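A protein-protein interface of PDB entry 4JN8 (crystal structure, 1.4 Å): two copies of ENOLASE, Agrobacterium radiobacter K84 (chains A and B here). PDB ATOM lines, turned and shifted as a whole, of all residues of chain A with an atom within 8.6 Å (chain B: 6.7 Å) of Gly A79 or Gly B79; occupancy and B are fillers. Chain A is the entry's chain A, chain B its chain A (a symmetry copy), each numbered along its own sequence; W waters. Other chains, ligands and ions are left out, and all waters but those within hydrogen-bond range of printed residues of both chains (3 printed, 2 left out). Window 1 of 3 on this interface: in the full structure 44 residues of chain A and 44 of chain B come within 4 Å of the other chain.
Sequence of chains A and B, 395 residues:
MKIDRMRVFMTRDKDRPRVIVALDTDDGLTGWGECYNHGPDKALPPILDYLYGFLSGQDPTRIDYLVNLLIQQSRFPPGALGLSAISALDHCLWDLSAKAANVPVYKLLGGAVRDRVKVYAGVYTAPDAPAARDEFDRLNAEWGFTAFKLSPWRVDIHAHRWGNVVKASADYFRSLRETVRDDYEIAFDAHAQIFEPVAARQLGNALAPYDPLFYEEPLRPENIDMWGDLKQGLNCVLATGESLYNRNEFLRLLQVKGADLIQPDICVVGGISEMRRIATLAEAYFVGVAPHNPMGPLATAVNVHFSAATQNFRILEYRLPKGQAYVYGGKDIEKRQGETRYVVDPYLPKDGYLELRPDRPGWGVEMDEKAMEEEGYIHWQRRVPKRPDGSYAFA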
ATOM      1  N   HIS A  38       9.560 -11.233  -4.258  1.00  0.00           N
ATOM      2  CA  HIS A  38       9.365 -12.609  -4.683  1.00  0.00           C
ATOM      3  C   HIS A  38       8.179 -12.772  -5.616  1.00  0.00           C
ATOM      4  O   HIS A  38       8.235 -13.532  -6.561  1.00  0.00           O
ATOM      5  CB  HIS A  38       9.244 -13.523  -3.470  1.00  0.00           C
ATOM      6  CG  HIS A  38      10.562 -13.885  -2.890  1.00  0.00           C
ATOM      7  ND1 HIS A  38      11.486 -14.644  -3.577  1.00  0.00           N
ATOM      8  CD2 HIS A  38      11.143 -13.536  -1.726  1.00  0.00           C
ATOM      9  CE1 HIS A  38      12.573 -14.768  -2.840  1.00  0.00           C
ATOM     10  NE2 HIS A  38      12.394 -14.092  -1.720  1.00  0.00           N
ATOM     11  N   LEU A  44       3.649  -9.260   2.304  1.00  0.00           N
ATOM     12  CA  LEU A  44       4.705  -8.744   3.160  1.00  0.00           C
ATOM     13  C   LEU A  44       4.224  -7.880   4.329  1.00  0.00           C
ATOM     14  O   LEU A  44       4.690  -8.068   5.447  1.00  0.00           O
ATOM     15  CB  LEU A  44       5.778  -8.030   2.324  1.00  0.00           C
ATOM     16  CG  LEU A  44       6.538  -8.969   1.390  1.00  0.00           C
ATOM     17  CD1 LEU A  44       7.396  -8.154   0.413  1.00  0.00           C
ATOM     18  CD2 LEU A  44       7.402  -9.948   2.179  1.00  0.00           C
ATOM     19  N   ILE A  47       3.212 -10.020   7.295  1.00  0.00           N
ATOM     20  CA  ILE A  47       4.369 -10.675   7.893  1.00  0.00           C
ATOM     21  C   ILE A  47       5.109  -9.662   8.750  1.00  0.00           C
ATOM     22  O   ILE A  47       5.477  -9.930   9.892  1.00  0.00           O
ATOM     23  CB  ILE A  47       5.307 -11.248   6.817  1.00  0.00           C
ATOM     24  CG1 ILE A  47       4.601 -12.344   6.007  1.00  0.00           C
ATOM     25  CG2 ILE A  47       6.561 -11.786   7.457  1.00  0.00           C
ATOM     26  CD1 ILE A  47       5.354 -12.762   4.754  1.00  0.00           C
ATOM     27  N   SER A  74       9.832 -18.377  14.403  1.00  0.00           N
ATOM     28  CA  SER A  74       9.080 -19.200  13.459  1.00  0.00           C
ATOM     29  C   SER A  74       9.322 -20.703  13.650  1.00  0.00           C
ATOM     30  O   SER A  74       8.500 -21.518  13.225  1.00  0.00           O
ATOM     31  CB  SER A  74       9.403 -18.810  12.036  1.00  0.00           C
ATOM     32  OG  SER A  74      10.748 -19.097  11.769  1.00  0.00           O
ATOM     33  N   PHE A  76      10.342 -23.313  12.390  1.00  0.00           N
ATOM     34  CA  PHE A  76      10.629 -23.739  11.024  1.00  0.00           C
ATOM     35  C   PHE A  76      11.573 -22.735  10.381  1.00  0.00           C
ATOM     36  O   PHE A  76      11.466 -21.536  10.635  1.00  0.00           O
ATOM     37  CB  PHE A  76       9.325 -23.757  10.224  1.00  0.00           C
ATOM     38  CG  PHE A  76       8.356 -24.822  10.650  1.00  0.00           C
ATOM     39  CD1 PHE A  76       7.541 -24.658  11.753  1.00  0.00           C
ATOM     40  CD2 PHE A  76       8.244 -25.983   9.924  1.00  0.00           C
ATOM     41  CE1 PHE A  76       6.665 -25.657  12.139  1.00  0.00           C
ATOM     42  CE2 PHE A  76       7.364 -26.974  10.303  1.00  0.00           C
ATOM     43  CZ  PHE A  76       6.572 -26.811  11.406  1.00  0.00           C
ATOM     44  N   PRO A  77      12.491 -23.184   9.513  1.00  0.00           N
ATOM     45  CA  PRO A  77      13.293 -22.202   8.769  1.00  0.00           C
ATOM     46  C   PRO A  77      12.415 -21.341   7.902  1.00  0.00           C
ATOM     47  O   PRO A  77      11.587 -21.844   7.131  1.00  0.00           O
ATOM     48  CB  PRO A  77      14.213 -23.056   7.895  1.00  0.00           C
ATOM     49  CG  PRO A  77      14.260 -24.384   8.592  1.00  0.00           C
ATOM     50  CD  PRO A  77      12.914 -24.567   9.232  1.00  0.00           C
ATOM     51  N   PRO A  78      12.585 -20.026   8.021  1.00  0.00           N
ATOM     52  CA  PRO A  78      11.716 -19.152   7.262  1.00  0.00           C
ATOM     53  C   PRO A  78      12.049 -19.317   5.813  1.00  0.00           C
ATOM     54  O   PRO A  78      13.192 -19.627   5.474  1.00  0.00           O
ATOM     55  CB  PRO A  78      12.069 -17.762   7.803  1.00  0.00           C
ATOM     56  CG  PRO A  78      13.397 -17.899   8.385  1.00  0.00           C
ATOM     57  CD  PRO A  78      13.501 -19.288   8.898  1.00  0.00           C
ATOM     58  N   GLY A  79      11.059 -19.177   4.962  1.00  0.00           N
ATOM     59  CA  GLY A  79      11.352 -19.277   3.559  1.00  0.00           C
ATOM     60  C   GLY A  79      11.506 -17.946   2.875  1.00  0.00           C
ATOM     61  O   GLY A  79      11.803 -16.929   3.487  1.00  0.00           O
ATOM     62  N   ALA A  80      11.244 -17.978   1.582  1.00  0.00           N
ATOM     63  CA  ALA A  80      11.325 -16.799   0.740  1.00  0.00           C
ATOM     64  C   ALA A  80      10.626 -15.585   1.343  1.00  0.00           C
ATOM     65  O   ALA A  80      11.236 -14.554   1.548  1.00  0.00           O
ATOM     66  CB  ALA A  80      10.747 -17.102  -0.594  1.00  0.00           C
ATOM     67  N   LEU A  81       9.329 -15.669   1.585  1.00  0.00           N
ATOM     68  CA  LEU A  81       8.592 -14.473   1.966  1.00  0.00           C
ATOM     69  C   LEU A  81       8.972 -13.999   3.352  1.00  0.00           C
ATOM     70  O   LEU A  81       9.209 -12.813   3.578  1.00  0.00           O
ATOM     71  CB  LEU A  81       7.078 -14.711   1.852  1.00  0.00           C
ATOM     72  CG  LEU A  81       6.612 -14.913   0.404  1.00  0.00           C
ATOM     73  CD1 LEU A  81       5.193 -15.475   0.410  1.00  0.00           C
ATOM     74  CD2 LEU A  81       6.666 -13.598  -0.371  1.00  0.00           C
ATOM     75  N   GLY A  82       9.020 -14.919   4.305  1.00  0.00           N
ATOM     76  CA  GLY A  82       9.434 -14.569   5.643  1.00  0.00           C
ATOM     77  C   GLY A  82      10.810 -13.941   5.705  1.00  0.00           C
ATOM     78  O   GLY A  82      11.020 -12.950   6.417  1.00  0.00           O
ATOM     79  N   LEU A  83      11.777 -14.516   4.998  1.00  0.00           N
ATOM     80  CA  LEU A  83      13.128 -13.972   5.005  1.00  0.00           C
ATOM     81  C   LEU A  83      13.242 -12.646   4.271  1.00  0.00           C
ATOM     82  O   LEU A  83      14.109 -11.843   4.586  1.00  0.00           O
ATOM     83  CB  LEU A  83      14.144 -14.960   4.425  1.00  0.00           C
ATOM     84  CG  LEU A  83      14.647 -16.043   5.369  1.00  0.00           C
ATOM     85  CD1 LEU A  83      15.513 -17.013   4.567  1.00  0.00           C
ATOM     86  CD2 LEU A  83      15.405 -15.441   6.540  1.00  0.00           C
ATOM     87  N   SER A  84      12.392 -12.418   3.280  1.00  0.00           N
ATOM     88  CA  SER A  84      12.380 -11.123   2.619  1.00  0.00           C
ATOM     89  C   SER A  84      12.028 -10.038   3.635  1.00  0.00           C
ATOM     90  O   SER A  84      12.679  -8.993   3.724  1.00  0.00           O
ATOM     91  CB  SER A  84      11.388 -11.107   1.463  1.00  0.00           C
ATOM     92  OG  SER A  84      11.314  -9.809   0.910  1.00  0.00           O
ATOM     93  N   ALA A  85      10.988 -10.287   4.412  1.00  0.00           N
ATOM     94  CA  ALA A  85      10.567  -9.335   5.443  1.00  0.00           C
ATOM     95  C   ALA A  85      11.655  -9.177   6.517  1.00  0.00           C
ATOM     96  O   ALA A  85      11.993  -8.063   6.929  1.00  0.00           O
ATOM     97  CB  ALA A  85       9.278  -9.802   6.089  1.00  0.00           C
ATOM     98  N   ILE A  86      12.232 -10.296   6.967  1.00  0.00           N
ATOM     99  CA  ILE A  86      13.314 -10.237   7.933  1.00  0.00           C
ATOM    100  C   ILE A  86      14.487  -9.422   7.383  1.00  0.00           C
ATOM    101  O   ILE A  86      15.085  -8.635   8.115  1.00  0.00           O
ATOM    102  CB  ILE A  86      13.764 -11.657   8.378  1.00  0.00           C
ATOM    103  CG1 ILE A  86      12.646 -12.287   9.214  1.00  0.00           C
ATOM    104  CG2 ILE A  86      15.062 -11.574   9.175  1.00  0.00           C
ATOM    105  CD1 ILE A  86      12.868 -13.755   9.563  1.00  0.00           C
ATOM    106  N   SER A  87      14.786  -9.585   6.099  1.00  0.00           N
ATOM    107  CA  SER A  87      15.877  -8.839   5.475  1.00  0.00           C
ATOM    108  C   SER A  87      15.671  -7.346   5.642  1.00  0.00           C
ATOM    109  O   SER A  87      16.587  -6.645   6.045  1.00  0.00           O
ATOM    110  CB  SER A  87      16.011  -9.168   3.988  1.00  0.00           C
ATOM    111  OG  SER A  87      16.355 -10.535   3.777  1.00  0.00           O
ATOM    112  N   TYR A 245      19.204 -19.586   0.834  1.00  0.00           N
ATOM    113  CA  TYR A 245      18.646 -18.705   1.861  1.00  0.00           C
ATOM    114  C   TYR A 245      19.455 -18.500   3.113  1.00  0.00           C
ATOM    115  O   TYR A 245      19.246 -17.507   3.817  1.00  0.00           O
ATOM    116  CB  TYR A 245      17.274 -19.230   2.305  1.00  0.00           C
ATOM    117  CG  TYR A 245      16.251 -19.192   1.220  1.00  0.00           C
ATOM    118  CD1 TYR A 245      15.789 -17.990   0.737  1.00  0.00           C
ATOM    119  CD2 TYR A 245      15.748 -20.364   0.665  1.00  0.00           C
ATOM    120  CE1 TYR A 245      14.858 -17.945  -0.265  1.00  0.00           C
ATOM    121  CE2 TYR A 245      14.801 -20.316  -0.350  1.00  0.00           C
ATOM    122  CZ  TYR A 245      14.375 -19.099  -0.807  1.00  0.00           C
ATOM    123  OH  TYR A 245      13.445 -19.019  -1.830  1.00  0.00           O
ATOM    124  N   ASN A 246      20.335 -19.430   3.461  1.00  0.00           N
ATOM    125  CA  ASN A 246      20.955 -19.351   4.780  1.00  0.00           C
ATOM    126  C   ASN A 246      22.343 -19.946   4.812  1.00  0.00           C
ATOM    127  O   ASN A 246      22.793 -20.571   3.850  1.00  0.00           O
ATOM    128  CB  ASN A 246      20.052 -19.978   5.852  1.00  0.00           C
ATOM    129  CG  ASN A 246      19.841 -21.462   5.660  1.00  0.00           C
ATOM    130  OD1 ASN A 246      20.775 -22.199   5.341  1.00  0.00           O
ATOM    131  ND2 ASN A 246      18.604 -21.918   5.848  1.00  0.00           N
ATOM    132  N   GLU A 249      22.667 -23.757   3.779  1.00  0.00           N
ATOM    133  CA  GLU A 249      22.570 -24.078   2.362  1.00  0.00           C
ATOM    134  C   GLU A 249      23.873 -23.704   1.656  1.00  0.00           C
ATOM    135  O   GLU A 249      24.407 -24.470   0.846  1.00  0.00           O
ATOM    136  CB  GLU A 249      21.366 -23.381   1.728  1.00  0.00           C
ATOM    137  CG  GLU A 249      20.058 -23.950   2.261  1.00  0.00           C
ATOM    138  CD  GLU A 249      18.809 -23.361   1.658  1.00  0.00           C
ATOM    139  OE1 GLU A 249      18.872 -22.422   0.847  1.00  0.00           O
ATOM    140  OE2 GLU A 249      17.717 -23.889   1.974  1.00  0.00           O
ATOM    141  N   CYS A 267      18.633  -9.011   0.203  1.00  0.00           N
ATOM    142  CA  CYS A 267      17.199  -8.851   0.445  1.00  0.00           C
ATOM    143  C   CYS A 267      16.447 -10.183   0.549  1.00  0.00           C
ATOM    144  O   CYS A 267      15.238 -10.194   0.770  1.00  0.00           O
ATOM    145  CB  CYS A 267      16.550  -8.039  -0.674  1.00  0.00           C
ATOM    146  SG  CYS A 267      17.147  -6.342  -0.844  1.00  0.00           S
ATOM    147  N   VAL A 268      17.172 -11.283   0.373  1.00  0.00           N
ATOM    148  CA  VAL A 268      16.616 -12.635   0.344  1.00  0.00           C
ATOM    149  C   VAL A 268      17.059 -13.473   1.538  1.00  0.00           C
ATOM    150  O   VAL A 268      16.260 -14.236   2.081  1.00  0.00           O
ATOM    151  CB  VAL A 268      17.027 -13.361  -0.963  1.00  0.00           C
ATOM    152  CG1 VAL A 268      16.704 -14.837  -0.940  1.00  0.00           C
ATOM    153  CG2 VAL A 268      16.384 -12.674  -2.166  1.00  0.00           C
ATOM    154  N   VAL A 269      18.317 -13.349   1.950  1.00  0.00           N
ATOM    155  CA  VAL A 269      18.912 -14.259   2.944  1.00  0.00           C
ATOM    156  C   VAL A 269      18.661 -13.854   4.386  1.00  0.00           C
ATOM    157  O   VAL A 269      19.056 -14.580   5.299  1.00  0.00           O
ATOM    158  CB  VAL A 269      20.455 -14.442   2.747  1.00  0.00           C
ATOM    159  CG1 VAL A 269      20.745 -15.007   1.383  1.00  0.00           C
ATOM    160  CG2 VAL A 269      21.205 -13.159   2.978  1.00  0.00           C
ATOM    161  N   GLY A 270      18.030 -12.704   4.613  1.00  0.00           N
ATOM    162  CA  GLY A 270      17.876 -12.184   5.960  1.00  0.00           C
ATOM    163  C   GLY A 270      18.778 -11.005   6.276  1.00  0.00           C
ATOM    164  O   GLY A 270      19.043 -10.716   7.423  1.00  0.00           O
ATOM    165  N   HIS B  38       1.893 -21.389  10.344  1.00  0.00           N
ATOM    166  CA  HIS B  38       3.256 -21.019  10.683  1.00  0.00           C
ATOM    167  C   HIS B  38       3.322 -19.892  11.698  1.00  0.00           C
ATOM    168  O   HIS B  38       4.160 -19.900  12.578  1.00  0.00           O
ATOM    169  CB  HIS B  38       4.039 -20.673   9.421  1.00  0.00           C
ATOM    170  CG  HIS B  38       4.538 -21.875   8.708  1.00  0.00           C
ATOM    171  ND1 HIS B  38       5.479 -22.720   9.258  1.00  0.00           N
ATOM    172  CD2 HIS B  38       4.181 -22.417   7.528  1.00  0.00           C
ATOM    173  CE1 HIS B  38       5.698 -23.720   8.426  1.00  0.00           C
ATOM    174  NE2 HIS B  38       4.911 -23.565   7.377  1.00  0.00           N
ATOM    175  N   PHE B  76      12.516 -19.121  -7.140  1.00  0.00           N
ATOM    176  CA  PHE B  76      13.093 -19.438  -5.838  1.00  0.00           C
ATOM    177  C   PHE B  76      12.294 -20.568  -5.206  1.00  0.00           C
ATOM    178  O   PHE B  76      11.075 -20.626  -5.362  1.00  0.00           O
ATOM    179  CB  PHE B  76      12.987 -18.208  -4.935  1.00  0.00           C
ATOM    180  CG  PHE B  76      13.860 -17.060  -5.354  1.00  0.00           C
ATOM    181  CD1 PHE B  76      13.487 -16.202  -6.370  1.00  0.00           C
ATOM    182  CD2 PHE B  76      15.050 -16.826  -4.707  1.00  0.00           C
ATOM    183  CE1 PHE B  76      14.311 -15.159  -6.751  1.00  0.00           C
ATOM    184  CE2 PHE B  76      15.866 -15.781  -5.081  1.00  0.00           C
ATOM    185  CZ  PHE B  76      15.497 -14.945  -6.098  1.00  0.00           C
ATOM    186  N   PRO B  77      12.944 -21.468  -4.453  1.00  0.00           N
ATOM    187  CA  PRO B  77      12.155 -22.461  -3.710  1.00  0.00           C
ATOM    188  C   PRO B  77      11.251 -21.789  -2.712  1.00  0.00           C
ATOM    189  O   PRO B  77      11.691 -20.952  -1.913  1.00  0.00           O
ATOM    190  CB  PRO B  77      13.205 -23.301  -2.980  1.00  0.00           C
ATOM    191  CG  PRO B  77      14.462 -23.096  -3.773  1.00  0.00           C
ATOM    192  CD  PRO B  77      14.392 -21.695  -4.309  1.00  0.00           C
ATOM    193  N   PRO B  78       9.970 -22.148  -2.750  1.00  0.00           N
ATOM    194  CA  PRO B  78       9.045 -21.479  -1.859  1.00  0.00           C
ATOM    195  C   PRO B  78       9.378 -21.886  -0.459  1.00  0.00           C
ATOM    196  O   PRO B  78       9.879 -22.991  -0.240  1.00  0.00           O
ATOM    197  CB  PRO B  78       7.681 -21.998  -2.326  1.00  0.00           C
ATOM    198  CG  PRO B  78       7.961 -23.245  -3.026  1.00  0.00           C
ATOM    199  CD  PRO B  78       9.302 -23.100  -3.645  1.00  0.00           C
ATOM    200  N   GLY B  79       9.168 -20.993   0.480  1.00  0.00           N
ATOM    201  CA  GLY B  79       9.426 -21.368   1.843  1.00  0.00           C
ATOM    202  C   GLY B  79       8.194 -21.772   2.606  1.00  0.00           C
ATOM    203  O   GLY B  79       7.184 -22.175   2.046  1.00  0.00           O
ATOM    204  N   ALA B  80       8.297 -21.603   3.911  1.00  0.00           N
ATOM    205  CA  ALA B  80       7.217 -21.922   4.826  1.00  0.00           C
ATOM    206  C   ALA B  80       5.868 -21.374   4.373  1.00  0.00           C
ATOM    207  O   ALA B  80       4.923 -22.117   4.193  1.00  0.00           O
ATOM    208  CB  ALA B  80       7.543 -21.403   6.178  1.00  0.00           C
ATOM    209  N   LEU B  81       5.741 -20.065   4.236  1.00  0.00           N
ATOM    210  CA  LEU B  81       4.423 -19.493   4.005  1.00  0.00           C
ATOM    211  C   LEU B  81       3.894 -19.840   2.630  1.00  0.00           C
ATOM    212  O   LEU B  81       2.741 -20.237   2.471  1.00  0.00           O
ATOM    213  CB  LEU B  81       4.446 -17.972   4.229  1.00  0.00           C
ATOM    214  CG  LEU B  81       4.699 -17.587   5.692  1.00  0.00           C
ATOM    215  CD1 LEU B  81       5.046 -16.103   5.765  1.00  0.00           C
ATOM    216  CD2 LEU B  81       3.476 -17.896   6.553  1.00  0.00           C
ATOM    217  N   GLY B  82       4.728 -19.678   1.613  1.00  0.00           N
ATOM    218  CA  GLY B  82       4.332 -20.043   0.274  1.00  0.00           C
ATOM    219  C   GLY B  82       3.908 -21.490   0.142  1.00  0.00           C
ATOM    220  O   GLY B  82       2.902 -21.796  -0.512  1.00  0.00           O
ATOM    221  N   LEU B  83       4.675 -22.406   0.721  1.00  0.00           N
ATOM    222  CA  LEU B  83       4.335 -23.820   0.640  1.00  0.00           C
ATOM    223  C   LEU B  83       3.106 -24.188   1.456  1.00  0.00           C
ATOM    224  O   LEU B  83       2.415 -25.142   1.128  1.00  0.00           O
ATOM    225  CB  LEU B  83       5.505 -24.714   1.059  1.00  0.00           C
ATOM    226  CG  LEU B  83       6.567 -24.977   0.000  1.00  0.00           C
ATOM    227  CD1 LEU B  83       7.717 -25.741   0.655  1.00  0.00           C
ATOM    228  CD2 LEU B  83       5.986 -25.731  -1.183  1.00  0.00           C
ATOM    229  N   SER B  84       2.841 -23.456   2.528  1.00  0.00           N
ATOM    230  CA  SER B  84       1.618 -23.689   3.281  1.00  0.00           C
ATOM    231  C   SER B  84       0.412 -23.433   2.378  1.00  0.00           C
ATOM    232  O   SER B  84      -0.531 -24.227   2.311  1.00  0.00           O
ATOM    233  CB  SER B  84       1.555 -22.796   4.513  1.00  0.00           C
ATOM    234  OG  SER B  84       0.310 -22.961   5.163  1.00  0.00           O
ATOM    235  N   TYR B 245      11.105 -29.258   3.869  1.00  0.00           N
ATOM    236  CA  TYR B 245      10.068 -28.768   2.959  1.00  0.00           C
ATOM    237  C   TYR B 245       9.880 -29.506   1.661  1.00  0.00           C
ATOM    238  O   TYR B 245       8.811 -29.400   1.051  1.00  0.00           O
ATOM    239  CB  TYR B 245      10.349 -27.304   2.595  1.00  0.00           C
ATOM    240  CG  TYR B 245      10.253 -26.380   3.762  1.00  0.00           C
ATOM    241  CD1 TYR B 245       9.042 -26.142   4.368  1.00  0.00           C
ATOM    242  CD2 TYR B 245      11.382 -25.746   4.271  1.00  0.00           C
ATOM    243  CE1 TYR B 245       8.946 -25.304   5.445  1.00  0.00           C
ATOM    244  CE2 TYR B 245      11.282 -24.893   5.363  1.00  0.00           C
ATOM    245  CZ  TYR B 245      10.059 -24.691   5.941  1.00  0.00           C
ATOM    246  OH  TYR B 245       9.930 -23.861   7.041  1.00  0.00           O
ATOM    247  N   VAL B 268       2.663 -28.550   5.098  1.00  0.00           N
ATOM    248  CA  VAL B 268       3.917 -27.799   5.076  1.00  0.00           C
ATOM    249  C   VAL B 268       4.707 -28.022   3.791  1.00  0.00           C
ATOM    250  O   VAL B 268       5.298 -27.079   3.263  1.00  0.00           O
ATOM    251  CB  VAL B 268       4.803 -28.188   6.288  1.00  0.00           C
ATOM    252  CG1 VAL B 268       6.208 -27.644   6.185  1.00  0.00           C
ATOM    253  CG2 VAL B 268       4.132 -27.746   7.587  1.00  0.00           C
HETATM  254  O   HOH W   1      11.235 -22.222   4.521  1.00  0.00           O
HETATM  255  O   HOH W   2      12.232 -20.737   0.683  1.00  0.00           O
HETATM  256  O   HOH W   3       7.034 -20.976  10.804  1.00  0.00           O
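Water W2 lies within hydrogen-bond range of the backbone carbonyl oxygen (O) of Pro B77 (2.7 Å), the backbone NH (N) of Ala A80 (3.1 Å), the backbone NH (N) of Gly B79 (3.1 Å), the side-chain hydroxyl (OH) of Tyr A245 (3.3 Å) and the backbone carbonyl oxygen (O) of Pro B78 (3.4 Å). Water W1 lies within hydrogen-bond range of O of Pro A77, N of Ala B80, N of Gly A79, OH of Tyr B245 and O of Pro A78. Water W3 lies within hydrogen-bond range of a ring nitrogen (ND1) of His B38 and the backbone carbonyl oxygen of Ser A74.
Among the printed residues, pairs that only touch across the chains: His A38 with Phe B76, Ile A47 with Leu B81, Phe A76 with His B38, Phe A76 with Tyr B245, Gly A79 with Gly B79, Gly A79 with Ala B80, Ala A80 with Gly B79 and Tyr A245 with Phe B76.
Of the 23 printed residues of chain A, 7 touch a printed residue of chain B. Hydrophobic or aromatic side chains of chain B that line the printed part of chain A: His B38, Phe B76, Pro B77, Leu B81 and Tyr B245.
The backbone carbonyl oxygen (O) of Ala A80 lies close to a ring nitrogen (NE2) of His A38. The backbone carbonyl oxygen of Phe A76 sits at hydrogen-bond distance from the side-chain hydroxyl of Ser A74, 2.8 Å away. The backbone NH (N) of Tyr A245 is in hydrogen-bond range of the side-chain carboxylate (OE1) of Glu A249, 2.9 Å away. NE2 of His B38 sits close to O of Ala B80 (3.5 Å).
His A38 touches Phe B76, and with the chains exchanged Phe A76 touches His B38. Phe A76 touches Tyr B245, and with the chains exchanged Tyr A245 touches Phe B76. Gly A79 touches its own counterpart, Gly B79. Gly A79 touches Ala B80, and with the chains exchanged Ala A80 touches Gly B79. Of the 10 pairs that touch across the chains among the printed residues, 9 have their exchanged pair printed and touching as well.
The backbone carbonyl oxygen (O) of Pro A77 sits at hydrogen-bond distance from the side-chain hydroxyl (OH) of Tyr B245 (2.6 Å). O of Pro B77 is in hydrogen-bond range of OH of Tyr A245, at 2.6 Å.
Of chain B, only Gly B79 and Ala B80 come within 4 Å of Gly A79. Gly B79 touches two residues of chain A. Printed residues of chain B within 4 Å of Pro A77: Tyr B245 (2.6 Å). Of the printed residues of chain B, His A38 touches Phe B76. Printed residues of chain B within 4 Å of Ala A80: Gly B79. Glu A249 touches none of the printed residues of chain B.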
